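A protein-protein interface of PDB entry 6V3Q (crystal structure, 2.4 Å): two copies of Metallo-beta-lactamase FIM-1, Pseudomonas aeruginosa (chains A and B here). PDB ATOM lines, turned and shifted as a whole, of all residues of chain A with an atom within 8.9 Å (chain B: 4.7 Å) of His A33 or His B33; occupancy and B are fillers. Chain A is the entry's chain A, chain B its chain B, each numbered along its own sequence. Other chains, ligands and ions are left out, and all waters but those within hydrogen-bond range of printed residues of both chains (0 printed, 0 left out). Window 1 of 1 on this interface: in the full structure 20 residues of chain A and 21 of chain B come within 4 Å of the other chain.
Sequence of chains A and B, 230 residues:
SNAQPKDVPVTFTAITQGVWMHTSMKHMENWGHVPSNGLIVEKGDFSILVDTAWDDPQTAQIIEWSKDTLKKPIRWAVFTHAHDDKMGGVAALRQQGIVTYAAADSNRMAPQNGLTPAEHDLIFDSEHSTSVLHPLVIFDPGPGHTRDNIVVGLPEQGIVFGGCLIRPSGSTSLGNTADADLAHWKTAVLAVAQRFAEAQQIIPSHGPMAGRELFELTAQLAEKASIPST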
ATOM      1  N   ALA A   3       5.401 -12.952  -8.322  1.00  0.00           N
ATOM      2  CA  ALA A   3       4.365 -11.947  -8.110  1.00  0.00           C
ATOM      3  C   ALA A   3       3.791 -12.052  -6.703  1.00  0.00           C
ATOM      4  O   ALA A   3       3.708 -11.059  -5.979  1.00  0.00           O
ATOM      5  CB  ALA A   3       3.261 -12.096  -9.147  1.00  0.00           C
ATOM      6  N   GLN A   4       3.390 -13.262  -6.321  1.00  0.00           N
ATOM      7  CA  GLN A   4       2.885 -13.535  -4.982  1.00  0.00           C
ATOM      8  C   GLN A   4       3.891 -14.404  -4.237  1.00  0.00           C
ATOM      9  O   GLN A   4       3.700 -15.623  -4.136  1.00  0.00           O
ATOM     10  CB  GLN A   4       1.524 -14.231  -5.043  1.00  0.00           C
ATOM     11  CG  GLN A   4       0.367 -13.322  -5.411  1.00  0.00           C
ATOM     12  CD  GLN A   4      -0.926 -14.085  -5.600  1.00  0.00           C
ATOM     13  OE1 GLN A   4      -1.163 -14.672  -6.656  1.00  0.00           O
ATOM     14  NE2 GLN A   4      -1.773 -14.080  -4.577  1.00  0.00           N
ATOM     15  N   PRO A   5       4.965 -13.822  -3.707  1.00  0.00           N
ATOM     16  CA  PRO A   5       6.009 -14.643  -3.089  1.00  0.00           C
ATOM     17  C   PRO A   5       5.556 -15.193  -1.748  1.00  0.00           C
ATOM     18  O   PRO A   5       4.846 -14.528  -0.990  1.00  0.00           O
ATOM     19  CB  PRO A   5       7.184 -13.667  -2.924  1.00  0.00           C
ATOM     20  CG  PRO A   5       6.783 -12.411  -3.673  1.00  0.00           C
ATOM     21  CD  PRO A   5       5.293 -12.391  -3.641  1.00  0.00           C
ATOM     22  N   LYS A   6       5.979 -16.424  -1.457  1.00  0.00           N
ATOM     23  CA  LYS A   6       5.641 -17.024  -0.171  1.00  0.00           C
ATOM     24  C   LYS A   6       6.441 -16.384   0.957  1.00  0.00           C
ATOM     25  O   LYS A   6       5.889 -16.056   2.014  1.00  0.00           O
ATOM     26  CB  LYS A   6       5.877 -18.535  -0.208  1.00  0.00           C
ATOM     27  CG  LYS A   6       5.343 -19.251   1.023  1.00  0.00           C
ATOM     28  CD  LYS A   6       5.796 -20.700   1.095  1.00  0.00           C
ATOM     29  CE  LYS A   6       5.214 -21.383   2.324  1.00  0.00           C
ATOM     30  NZ  LYS A   6       5.853 -22.697   2.602  1.00  0.00           N
ATOM     31  N   ASP A   7       7.743 -16.191   0.750  1.00  0.00           N
ATOM     32  CA  ASP A   7       8.633 -15.641   1.766  1.00  0.00           C
ATOM     33  C   ASP A   7       9.200 -14.316   1.277  1.00  0.00           C
ATOM     34  O   ASP A   7       9.822 -14.257   0.211  1.00  0.00           O
ATOM     35  CB  ASP A   7       9.759 -16.622   2.096  1.00  0.00           C
ATOM     36  CG  ASP A   7       9.242 -18.002   2.454  1.00  0.00           C
ATOM     37  OD1 ASP A   7       9.383 -18.927   1.628  1.00  0.00           O
ATOM     38  OD2 ASP A   7       8.682 -18.163   3.557  1.00  0.00           O
ATOM     39  N   VAL A   8       8.990 -13.262   2.061  1.00  0.00           N
ATOM     40  CA  VAL A   8       9.458 -11.917   1.734  1.00  0.00           C
ATOM     41  C   VAL A   8      10.611 -11.556   2.665  1.00  0.00           C
ATOM     42  O   VAL A   8      10.552 -11.857   3.866  1.00  0.00           O
ATOM     43  CB  VAL A   8       8.305 -10.902   1.827  1.00  0.00           C
ATOM     44  CG1 VAL A   8       7.336 -11.312   2.922  1.00  0.00           C
ATOM     45  CG2 VAL A   8       8.828  -9.491   2.073  1.00  0.00           C
ATOM     46  N   PRO A   9      11.676 -10.934   2.161  1.00  0.00           N
ATOM     47  CA  PRO A   9      12.811 -10.594   3.027  1.00  0.00           C
ATOM     48  C   PRO A   9      12.445  -9.574   4.096  1.00  0.00           C
ATOM     49  O   PRO A   9      11.547  -8.746   3.924  1.00  0.00           O
ATOM     50  CB  PRO A   9      13.847 -10.021   2.048  1.00  0.00           C
ATOM     51  CG  PRO A   9      13.065  -9.637   0.832  1.00  0.00           C
ATOM     52  CD  PRO A   9      11.942 -10.619   0.747  1.00  0.00           C
ATOM     53  N   SER A  24       9.298  -8.154   9.807  1.00  0.00           N
ATOM     54  CA  SER A  24       9.276  -9.455   9.159  1.00  0.00           C
ATOM     55  C   SER A  24       7.834  -9.913   9.001  1.00  0.00           C
ATOM     56  O   SER A  24       6.967  -9.572   9.809  1.00  0.00           O
ATOM     57  CB  SER A  24      10.078 -10.488   9.961  1.00  0.00           C
ATOM     58  OG  SER A  24       9.612 -10.576  11.297  1.00  0.00           O
ATOM     59  N   MET A  25       7.583 -10.693   7.956  1.00  0.00           N
ATOM     60  CA  MET A  25       6.241 -11.151   7.629  1.00  0.00           C
ATOM     61  C   MET A  25       6.119 -12.649   7.872  1.00  0.00           C
ATOM     62  O   MET A  25       7.030 -13.419   7.547  1.00  0.00           O
ATOM     63  CB  MET A  25       5.891 -10.833   6.173  1.00  0.00           C
ATOM     64  CG  MET A  25       6.276  -9.421   5.746  1.00  0.00           C
ATOM     65  SD  MET A  25       5.458  -8.139   6.711  1.00  0.00           S
ATOM     66  CE  MET A  25       3.773  -8.259   6.111  1.00  0.00           C
ATOM     67  N   LYS A  26       4.991 -13.054   8.451  1.00  0.00           N
ATOM     68  CA  LYS A  26       4.650 -14.461   8.597  1.00  0.00           C
ATOM     69  C   LYS A  26       3.662 -14.838   7.503  1.00  0.00           C
ATOM     70  O   LYS A  26       2.634 -14.173   7.331  1.00  0.00           O
ATOM     71  CB  LYS A  26       4.055 -14.752   9.975  1.00  0.00           C
ATOM     72  CG  LYS A  26       4.194 -16.207  10.401  1.00  0.00           C
ATOM     73  CD  LYS A  26       2.893 -16.762  10.962  1.00  0.00           C
ATOM     74  CE  LYS A  26       2.247 -15.796  11.939  1.00  0.00           C
ATOM     75  NZ  LYS A  26       1.116 -16.401  12.690  1.00  0.00           N
ATOM     76  N   HIS A  27       3.991 -15.886   6.753  1.00  0.00           N
ATOM     77  CA  HIS A  27       3.101 -16.381   5.714  1.00  0.00           C
ATOM     78  C   HIS A  27       1.932 -17.124   6.346  1.00  0.00           C
ATOM     79  O   HIS A  27       2.124 -17.988   7.209  1.00  0.00           O
ATOM     80  CB  HIS A  27       3.871 -17.291   4.754  1.00  0.00           C
ATOM     81  CG  HIS A  27       2.997 -18.156   3.898  1.00  0.00           C
ATOM     82  ND1 HIS A  27       2.392 -17.699   2.747  1.00  0.00           N
ATOM     83  CD2 HIS A  27       2.638 -19.455   4.023  1.00  0.00           C
ATOM     84  CE1 HIS A  27       1.693 -18.679   2.202  1.00  0.00           C
ATOM     85  NE2 HIS A  27       1.823 -19.755   2.958  1.00  0.00           N
ATOM     86  N   MET A  28       0.722 -16.799   5.915  1.00  0.00           N
ATOM     87  CA  MET A  28      -0.480 -17.446   6.417  1.00  0.00           C
ATOM     88  C   MET A  28      -1.055 -18.371   5.350  1.00  0.00           C
ATOM     89  O   MET A  28      -0.652 -18.343   4.184  1.00  0.00           O
ATOM     90  CB  MET A  28      -1.511 -16.402   6.863  1.00  0.00           C
ATOM     91  CG  MET A  28      -0.956 -15.383   7.860  1.00  0.00           C
ATOM     92  SD  MET A  28      -1.372 -15.694   9.592  1.00  0.00           S
ATOM     93  CE  MET A  28      -0.525 -17.239   9.917  1.00  0.00           C
ATOM     94  N   GLU A  29      -2.004 -19.211   5.771  1.00  0.00           N
ATOM     95  CA  GLU A  29      -2.551 -20.216   4.860  1.00  0.00           C
ATOM     96  C   GLU A  29      -3.382 -19.592   3.747  1.00  0.00           C
ATOM     97  O   GLU A  29      -3.456 -20.155   2.648  1.00  0.00           O
ATOM     98  CB  GLU A  29      -3.387 -21.245   5.625  1.00  0.00           C
ATOM     99  CG  GLU A  29      -2.589 -22.434   6.141  1.00  0.00           C
ATOM    100  CD  GLU A  29      -3.453 -23.665   6.345  1.00  0.00           C
ATOM    101  OE1 GLU A  29      -4.558 -23.724   5.766  1.00  0.00           O
ATOM    102  OE2 GLU A  29      -3.025 -24.579   7.079  1.00  0.00           O
ATOM    103  N   ASN A  30      -4.009 -18.445   3.997  1.00  0.00           N
ATOM    104  CA  ASN A  30      -4.699 -17.731   2.930  1.00  0.00           C
ATOM    105  C   ASN A  30      -3.742 -16.923   2.063  1.00  0.00           C
ATOM    106  O   ASN A  30      -4.196 -16.089   1.269  1.00  0.00           O
ATOM    107  CB  ASN A  30      -5.789 -16.819   3.507  1.00  0.00           C
ATOM    108  CG  ASN A  30      -5.252 -15.818   4.517  1.00  0.00           C
ATOM    109  OD1 ASN A  30      -4.053 -15.542   4.571  1.00  0.00           O
ATOM    110  ND2 ASN A  30      -6.149 -15.262   5.319  1.00  0.00           N
ATOM    111  N   TRP A  31      -2.437 -17.149   2.211  1.00  0.00           N
ATOM    112  CA  TRP A  31      -1.359 -16.504   1.468  1.00  0.00           C
ATOM    113  C   TRP A  31      -1.260 -15.011   1.730  1.00  0.00           C
ATOM    114  O   TRP A  31      -0.613 -14.295   0.957  1.00  0.00           O
ATOM    115  CB  TRP A  31      -1.472 -16.769  -0.033  1.00  0.00           C
ATOM    116  CG  TRP A  31      -0.964 -18.116  -0.372  1.00  0.00           C
ATOM    117  CD1 TRP A  31      -1.604 -19.305  -0.181  1.00  0.00           C
ATOM    118  CD2 TRP A  31       0.313 -18.431  -0.933  1.00  0.00           C
ATOM    119  NE1 TRP A  31      -0.808 -20.341  -0.605  1.00  0.00           N
ATOM    120  CE2 TRP A  31       0.375 -19.830  -1.069  1.00  0.00           C
ATOM    121  CE3 TRP A  31       1.407 -17.662  -1.340  1.00  0.00           C
ATOM    122  CZ2 TRP A  31       1.488 -20.479  -1.595  1.00  0.00           C
ATOM    123  CZ3 TRP A  31       2.510 -18.307  -1.863  1.00  0.00           C
ATOM    124  CH2 TRP A  31       2.543 -19.701  -1.985  1.00  0.00           C
ATOM    125  N   GLY A  32      -1.872 -14.520   2.799  1.00  0.00           N
ATOM    126  CA  GLY A  32      -1.568 -13.200   3.292  1.00  0.00           C
ATOM    127  C   GLY A  32      -0.338 -13.219   4.172  1.00  0.00           C
ATOM    128  O   GLY A  32       0.279 -14.254   4.419  1.00  0.00           O
ATOM    129  N   HIS A  33       0.031 -12.034   4.648  1.00  0.00           N
ATOM    130  CA  HIS A  33       1.151 -11.896   5.564  1.00  0.00           C
ATOM    131  C   HIS A  33       0.718 -11.045   6.746  1.00  0.00           C
ATOM    132  O   HIS A  33      -0.141 -10.172   6.615  1.00  0.00           O
ATOM    133  CB  HIS A  33       2.377 -11.261   4.885  1.00  0.00           C
ATOM    134  CG  HIS A  33       2.994 -12.107   3.812  1.00  0.00           C
ATOM    135  ND1 HIS A  33       2.585 -12.061   2.496  1.00  0.00           N
ATOM    136  CD2 HIS A  33       4.004 -13.009   3.858  1.00  0.00           C
ATOM    137  CE1 HIS A  33       3.310 -12.902   1.781  1.00  0.00           C
ATOM    138  NE2 HIS A  33       4.178 -13.491   2.584  1.00  0.00           N
ATOM    139  N   VAL A  34       1.313 -11.311   7.906  1.00  0.00           N
ATOM    140  CA  VAL A  34       1.130 -10.502   9.103  1.00  0.00           C
ATOM    141  C   VAL A  34       2.492  -9.961   9.510  1.00  0.00           C
ATOM    142  O   VAL A  34       3.440 -10.739   9.644  1.00  0.00           O
ATOM    143  CB  VAL A  34       0.487 -11.285  10.265  1.00  0.00           C
ATOM    144  CG1 VAL A  34      -0.951 -11.641   9.935  1.00  0.00           C
ATOM    145  CG2 VAL A  34       1.268 -12.551  10.591  1.00  0.00           C
ATOM    146  N   PRO A  35       2.654  -8.652   9.680  1.00  0.00           N
ATOM    147  CA  PRO A  35       3.965  -8.098  10.024  1.00  0.00           C
ATOM    148  C   PRO A  35       4.223  -8.076  11.525  1.00  0.00           C
ATOM    149  O   PRO A  35       3.308  -8.126  12.349  1.00  0.00           O
ATOM    150  CB  PRO A  35       3.885  -6.669   9.471  1.00  0.00           C
ATOM    151  CG  PRO A  35       2.448  -6.315   9.628  1.00  0.00           C
ATOM    152  CD  PRO A  35       1.672  -7.591   9.389  1.00  0.00           C
ATOM    153  N   SER A  36       5.510  -8.000  11.862  1.00  0.00           N
ATOM    154  CA  SER A  36       5.949  -7.845  13.241  1.00  0.00           C
ATOM    155  C   SER A  36       7.166  -6.933  13.265  1.00  0.00           C
ATOM    156  O   SER A  36       8.066  -7.071  12.433  1.00  0.00           O
ATOM    157  CB  SER A  36       6.290  -9.192  13.891  1.00  0.00           C
ATOM    158  OG  SER A  36       6.597  -9.027  15.262  1.00  0.00           O
ATOM    159  N   TRP A  54       9.892 -13.931  13.027  1.00  0.00           N
ATOM    160  CA  TRP A  54       8.946 -15.003  13.316  1.00  0.00           C
ATOM    161  C   TRP A  54       9.637 -16.350  13.494  1.00  0.00           C
ATOM    162  O   TRP A  54       9.182 -17.171  14.300  1.00  0.00           O
ATOM    163  CB  TRP A  54       7.895 -15.089  12.210  1.00  0.00           C
ATOM    164  CG  TRP A  54       6.963 -13.914  12.173  1.00  0.00           C
ATOM    165  CD1 TRP A  54       7.111 -12.777  11.436  1.00  0.00           C
ATOM    166  CD2 TRP A  54       5.739 -13.761  12.905  1.00  0.00           C
ATOM    167  NE1 TRP A  54       6.058 -11.925  11.662  1.00  0.00           N
ATOM    168  CE2 TRP A  54       5.200 -12.505  12.560  1.00  0.00           C
ATOM    169  CE3 TRP A  54       5.045 -14.563  13.818  1.00  0.00           C
ATOM    170  CZ2 TRP A  54       4.001 -12.031  13.094  1.00  0.00           C
ATOM    171  CZ3 TRP A  54       3.855 -14.089  14.349  1.00  0.00           C
ATOM    172  CH2 TRP A  54       3.345 -12.837  13.984  1.00  0.00           C
ATOM    173  N   GLN A  58      14.450 -16.027   9.278  1.00  0.00           N
ATOM    174  CA  GLN A  58      14.196 -14.592   9.193  1.00  0.00           C
ATOM    175  C   GLN A  58      15.012 -13.828  10.228  1.00  0.00           C
ATOM    176  O   GLN A  58      15.502 -12.726   9.951  1.00  0.00           O
ATOM    177  CB  GLN A  58      12.703 -14.306   9.361  1.00  0.00           C
ATOM    178  CG  GLN A  58      11.904 -14.284   8.061  1.00  0.00           C
ATOM    179  CD  GLN A  58      10.438 -13.942   8.280  1.00  0.00           C
ATOM    180  OE1 GLN A  58       9.853 -14.296   9.303  1.00  0.00           O
ATOM    181  NE2 GLN A  58       9.840 -13.251   7.315  1.00  0.00           N
ATOM    182  N   HIS A 206       2.741  -4.175  15.525  1.00  0.00           N
ATOM    183  CA  HIS A 206       2.187  -4.269  14.184  1.00  0.00           C
ATOM    184  C   HIS A 206       1.926  -2.878  13.625  1.00  0.00           C
ATOM    185  O   HIS A 206       1.418  -1.999  14.329  1.00  0.00           O
ATOM    186  CB  HIS A 206       0.890  -5.076  14.186  1.00  0.00           C
ATOM    187  CG  HIS A 206       0.999  -6.379  14.911  1.00  0.00           C
ATOM    188  ND1 HIS A 206       1.994  -7.293  14.644  1.00  0.00           N
ATOM    189  CD2 HIS A 206       0.245  -6.917  15.898  1.00  0.00           C
ATOM    190  CE1 HIS A 206       1.846  -8.343  15.432  1.00  0.00           C
ATOM    191  NE2 HIS A 206       0.792  -8.140  16.202  1.00  0.00           N
ATOM    192  N   PRO B   5       2.713   0.323   3.604  1.00  0.00           N
ATOM    193  CA  PRO B   5       1.539   1.060   3.133  1.00  0.00           C
ATOM    194  C   PRO B   5       0.251   0.405   3.604  1.00  0.00           C
ATOM    195  O   PRO B   5       0.143  -0.822   3.687  1.00  0.00           O
ATOM    196  CB  PRO B   5       1.673   0.995   1.608  1.00  0.00           C
ATOM    197  CG  PRO B   5       2.348  -0.312   1.374  1.00  0.00           C
ATOM    198  CD  PRO B   5       3.284  -0.530   2.544  1.00  0.00           C
ATOM    199  N   LYS B   6      -0.730   1.245   3.924  1.00  0.00           N
ATOM    200  CA  LYS B   6      -2.032   0.731   4.335  1.00  0.00           C
ATOM    201  C   LYS B   6      -2.796   0.171   3.143  1.00  0.00           C
ATOM    202  O   LYS B   6      -3.382  -0.915   3.221  1.00  0.00           O
ATOM    203  CB  LYS B   6      -2.828   1.834   5.030  1.00  0.00           C
ATOM    204  CG  LYS B   6      -4.227   1.435   5.451  1.00  0.00           C
ATOM    205  CD  LYS B   6      -4.750   2.403   6.498  1.00  0.00           C
ATOM    206  CE  LYS B   6      -6.262   2.394   6.573  1.00  0.00           C
ATOM    207  NZ  LYS B   6      -6.756   3.574   7.331  1.00  0.00           N
ATOM    208  N   VAL B   8      -2.446  -0.988  -0.841  1.00  0.00           N
ATOM    209  CA  VAL B   8      -1.540  -1.378  -1.920  1.00  0.00           C
ATOM    210  C   VAL B   8      -2.359  -1.532  -3.197  1.00  0.00           C
ATOM    211  O   VAL B   8      -3.467  -2.086  -3.155  1.00  0.00           O
ATOM    212  CB  VAL B   8      -0.779  -2.665  -1.559  1.00  0.00           C
ATOM    213  CG1 VAL B   8      -1.669  -3.591  -0.748  1.00  0.00           C
ATOM    214  CG2 VAL B   8      -0.261  -3.374  -2.804  1.00  0.00           C
ATOM    215  N   MET B  25      -5.636  -6.652  -2.156  1.00  0.00           N
ATOM    216  CA  MET B  25      -5.316  -6.908  -0.759  1.00  0.00           C
ATOM    217  C   MET B  25      -6.311  -6.189   0.141  1.00  0.00           C
ATOM    218  O   MET B  25      -6.629  -5.016  -0.090  1.00  0.00           O
ATOM    219  CB  MET B  25      -3.890  -6.454  -0.440  1.00  0.00           C
ATOM    220  CG  MET B  25      -2.871  -6.833  -1.513  1.00  0.00           C
ATOM    221  SD  MET B  25      -2.691  -8.612  -1.728  1.00  0.00           S
ATOM    222  CE  MET B  25      -2.100  -9.102  -0.111  1.00  0.00           C
ATOM    223  N   LYS B  26      -6.806  -6.891   1.158  1.00  0.00           N
ATOM    224  CA  LYS B  26      -7.604  -6.279   2.210  1.00  0.00           C
ATOM    225  C   LYS B  26      -6.701  -5.968   3.396  1.00  0.00           C
ATOM    226  O   LYS B  26      -5.997  -6.851   3.897  1.00  0.00           O
ATOM    227  CB  LYS B  26      -8.754  -7.184   2.653  1.00  0.00           C
ATOM    228  CG  LYS B  26      -9.585  -6.562   3.768  1.00  0.00           C
ATOM    229  CD  LYS B  26     -10.848  -7.351   4.064  1.00  0.00           C
ATOM    230  CE  LYS B  26     -10.536  -8.735   4.604  1.00  0.00           C
ATOM    231  NZ  LYS B  26     -11.771  -9.441   5.050  1.00  0.00           N
ATOM    232  N   HIS B  27      -6.711  -4.709   3.822  1.00  0.00           N
ATOM    233  CA  HIS B  27      -5.974  -4.307   5.008  1.00  0.00           C
ATOM    234  C   HIS B  27      -6.660  -4.840   6.259  1.00  0.00           C
ATOM    235  O   HIS B  27      -7.881  -4.747   6.407  1.00  0.00           O
ATOM    236  CB  HIS B  27      -5.861  -2.783   5.064  1.00  0.00           C
ATOM    237  CG  HIS B  27      -5.471  -2.249   6.408  1.00  0.00           C
ATOM    238  ND1 HIS B  27      -4.159  -2.129   6.813  1.00  0.00           N
ATOM    239  CD2 HIS B  27      -6.224  -1.796   7.439  1.00  0.00           C
ATOM    240  CE1 HIS B  27      -4.119  -1.627   8.035  1.00  0.00           C
ATOM    241  NE2 HIS B  27      -5.360  -1.418   8.438  1.00  0.00           N
ATOM    242  N   MET B  28      -5.865  -5.410   7.159  1.00  0.00           N
ATOM    243  CA  MET B  28      -6.349  -5.959   8.417  1.00  0.00           C
ATOM    244  C   MET B  28      -5.941  -5.057   9.574  1.00  0.00           C
ATOM    245  O   MET B  28      -5.162  -4.115   9.413  1.00  0.00           O
ATOM    246  CB  MET B  28      -5.811  -7.375   8.633  1.00  0.00           C
ATOM    247  CG  MET B  28      -6.228  -8.365   7.560  1.00  0.00           C
ATOM    248  SD  MET B  28      -5.832 -10.064   8.019  1.00  0.00           S
ATOM    249  CE  MET B  28      -4.047 -10.013   8.042  1.00  0.00           C
ATOM    250  N   TRP B  31      -2.397  -4.865  10.559  1.00  0.00           N
ATOM    251  CA  TRP B  31      -1.693  -4.288   9.420  1.00  0.00           C
ATOM    252  C   TRP B  31      -1.141  -5.338   8.470  1.00  0.00           C
ATOM    253  O   TRP B  31      -0.293  -5.019   7.628  1.00  0.00           O
ATOM    254  CB  TRP B  31      -0.580  -3.338   9.867  1.00  0.00           C
ATOM    255  CG  TRP B  31      -1.139  -2.027  10.273  1.00  0.00           C
ATOM    256  CD1 TRP B  31      -1.796  -1.740  11.431  1.00  0.00           C
ATOM    257  CD2 TRP B  31      -1.125  -0.820   9.508  1.00  0.00           C
ATOM    258  NE1 TRP B  31      -2.180  -0.422  11.441  1.00  0.00           N
ATOM    259  CE2 TRP B  31      -1.781   0.165  10.270  1.00  0.00           C
ATOM    260  CE3 TRP B  31      -0.613  -0.474   8.254  1.00  0.00           C
ATOM    261  CZ2 TRP B  31      -1.940   1.472   9.820  1.00  0.00           C
ATOM    262  CZ3 TRP B  31      -0.772   0.824   7.808  1.00  0.00           C
ATOM    263  CH2 TRP B  31      -1.429   1.781   8.589  1.00  0.00           C
ATOM    264  N   GLY B  32      -1.602  -6.577   8.573  1.00  0.00           N
ATOM    265  CA  GLY B  32      -1.372  -7.549   7.534  1.00  0.00           C
ATOM    266  C   GLY B  32      -2.278  -7.293   6.346  1.00  0.00           C
ATOM    267  O   GLY B  32      -3.094  -6.371   6.322  1.00  0.00           O
ATOM    268  N   HIS B  33      -2.124  -8.135   5.331  1.00  0.00           N
ATOM    269  CA  HIS B  33      -2.929  -8.040   4.123  1.00  0.00           C
ATOM    270  C   HIS B  33      -3.396  -9.432   3.730  1.00  0.00           C
ATOM    271  O   HIS B  33      -2.667 -10.409   3.920  1.00  0.00           O
ATOM    272  CB  HIS B  33      -2.142  -7.395   2.968  1.00  0.00           C
ATOM    273  CG  HIS B  33      -2.040  -5.902   3.051  1.00  0.00           C
ATOM    274  ND1 HIS B  33      -0.904  -5.255   3.488  1.00  0.00           N
ATOM    275  CD2 HIS B  33      -2.929  -4.929   2.736  1.00  0.00           C
ATOM    276  CE1 HIS B  33      -1.100  -3.948   3.444  1.00  0.00           C
ATOM    277  NE2 HIS B  33      -2.321  -3.724   2.993  1.00  0.00           N
ATOM    278  N   VAL B  34      -4.607  -9.521   3.193  1.00  0.00           N
ATOM    279  CA  VAL B  34      -5.186 -10.776   2.731  1.00  0.00           C
ATOM    280  C   VAL B  34      -5.493 -10.644   1.243  1.00  0.00           C
ATOM    281  O   VAL B  34      -6.288  -9.786   0.849  1.00  0.00           O
ATOM    282  CB  VAL B  34      -6.456 -11.159   3.510  1.00  0.00           C
ATOM    283  CG1 VAL B  34      -7.235 -12.233   2.766  1.00  0.00           C
ATOM    284  CG2 VAL B  34      -6.089 -11.648   4.894  1.00  0.00           C
ATOM    285  N   PRO B  35      -4.899 -11.468   0.384  1.00  0.00           N
ATOM    286  CA  PRO B  35      -5.121 -11.341  -1.059  1.00  0.00           C
ATOM    287  C   PRO B  35      -6.377 -12.060  -1.529  1.00  0.00           C
ATOM    288  O   PRO B  35      -6.906 -12.958  -0.869  1.00  0.00           O
ATOM    289  CB  PRO B  35      -3.867 -12.000  -1.650  1.00  0.00           C
ATOM    290  CG  PRO B  35      -3.536 -13.066  -0.659  1.00  0.00           C
ATOM    291  CD  PRO B  35      -3.916 -12.519   0.700  1.00  0.00           C
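Trp A31 touches Pro B35, and with the chains exchanged Pro A35 touches Trp B31.
Gly A32 touches His B33, and with the chains exchanged His A33 touches Gly B32.
His B33 touches its own counterpart, His A33.
Val A34 touches Met B28, but with the chains exchanged Met A28 does not touch Val B34 (6.9 Å).
Of chain B, only Gly B32 (3.0 Å) and His B33 (3.1 Å) come within 4 Å of His A33.
Of the printed residues of chain B, Val A34 touches Met B28.
Printed residues of chain A within 4 Å of His B33: Gly A32 (3.1 Å) and His A33 (3.1 Å).
Printed residues of chain A within 4 Å of Val B34: Asn A30 (3.6 Å).
Printed residues of chain A within 4 Å of Pro B35: Asn A30, Trp A31 and Gly A32.
The nearest printed residue of chain B that does not touch His A33 is Met B28 (4.2 Å).
The nearest printed residue of chain A that does not touch His B33 is Trp A31 (5.3 Å).
The backbone NH (N) of His B33 lies within hydrogen-bond range of the backbone carbonyl oxygen (O) of His A33, 3.1 Å away.
Of the 12 printed residues of chain B, 6 touch a printed residue of chain A.
Hydrophobic or aromatic side chains of chain B that line the printed part of chain A: Met B28, Val B34 and Pro B35.
Printed residues of chain A that touch a printed residue of chain B: Asn A30, Trp A31, Gly A32, His A33, Val A34 and Pro A35.
Hydrophobic or aromatic side chains of chain A within 4 Å of the printed part of chain B: Val A34 and Pro A35.
Among the printed residues, 10 pairs touch across the chains.
The backbone carbonyl oxygen of Lys A6 sits at hydrogen-bond distance from a ring nitrogen (NE2) of His A33 (3.1 Å).
The backbone carbonyl oxygen (O) of Val A34 lies within hydrogen-bond range of the backbone NH (N) of Lys A26 (3.0 Å).
N of Gly A32 lies within hydrogen-bond range of OD1 of Asn A30, 3.0 Å away.
The backbone carbonyl oxygen (O) of Pro A35 lies within hydrogen-bond range of a ring nitrogen (ND1) of His A206 (2.8 Å).
The backbone carbonyl oxygen (O) of Lys B6 is in hydrogen-bond range of a ring nitrogen (NE2) of His B33, at 3.0 Å.
O of Val B34 is in hydrogen-bond range of N of Lys B26, 3.0 Å away.
Asn A30 touches Val B34.
O of Asn A30 touches CD of Pro B35 (3.6 Å).
Pro B35 touches Trp A31 (CG to O, 3.6 Å).
Gly A32 touches His B33 (CA to O, 3.1 Å).
Gly A32 touches Pro B35.
CA of Gly B32 touches O of His A33, 3.0 Å away.
CE of Met B28 touches CG1 of Val A34, 3.98 Å away.
Pro A35 touches Trp B31 (CG to O, 3.6 Å).
Pro A35 touches Gly B32.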
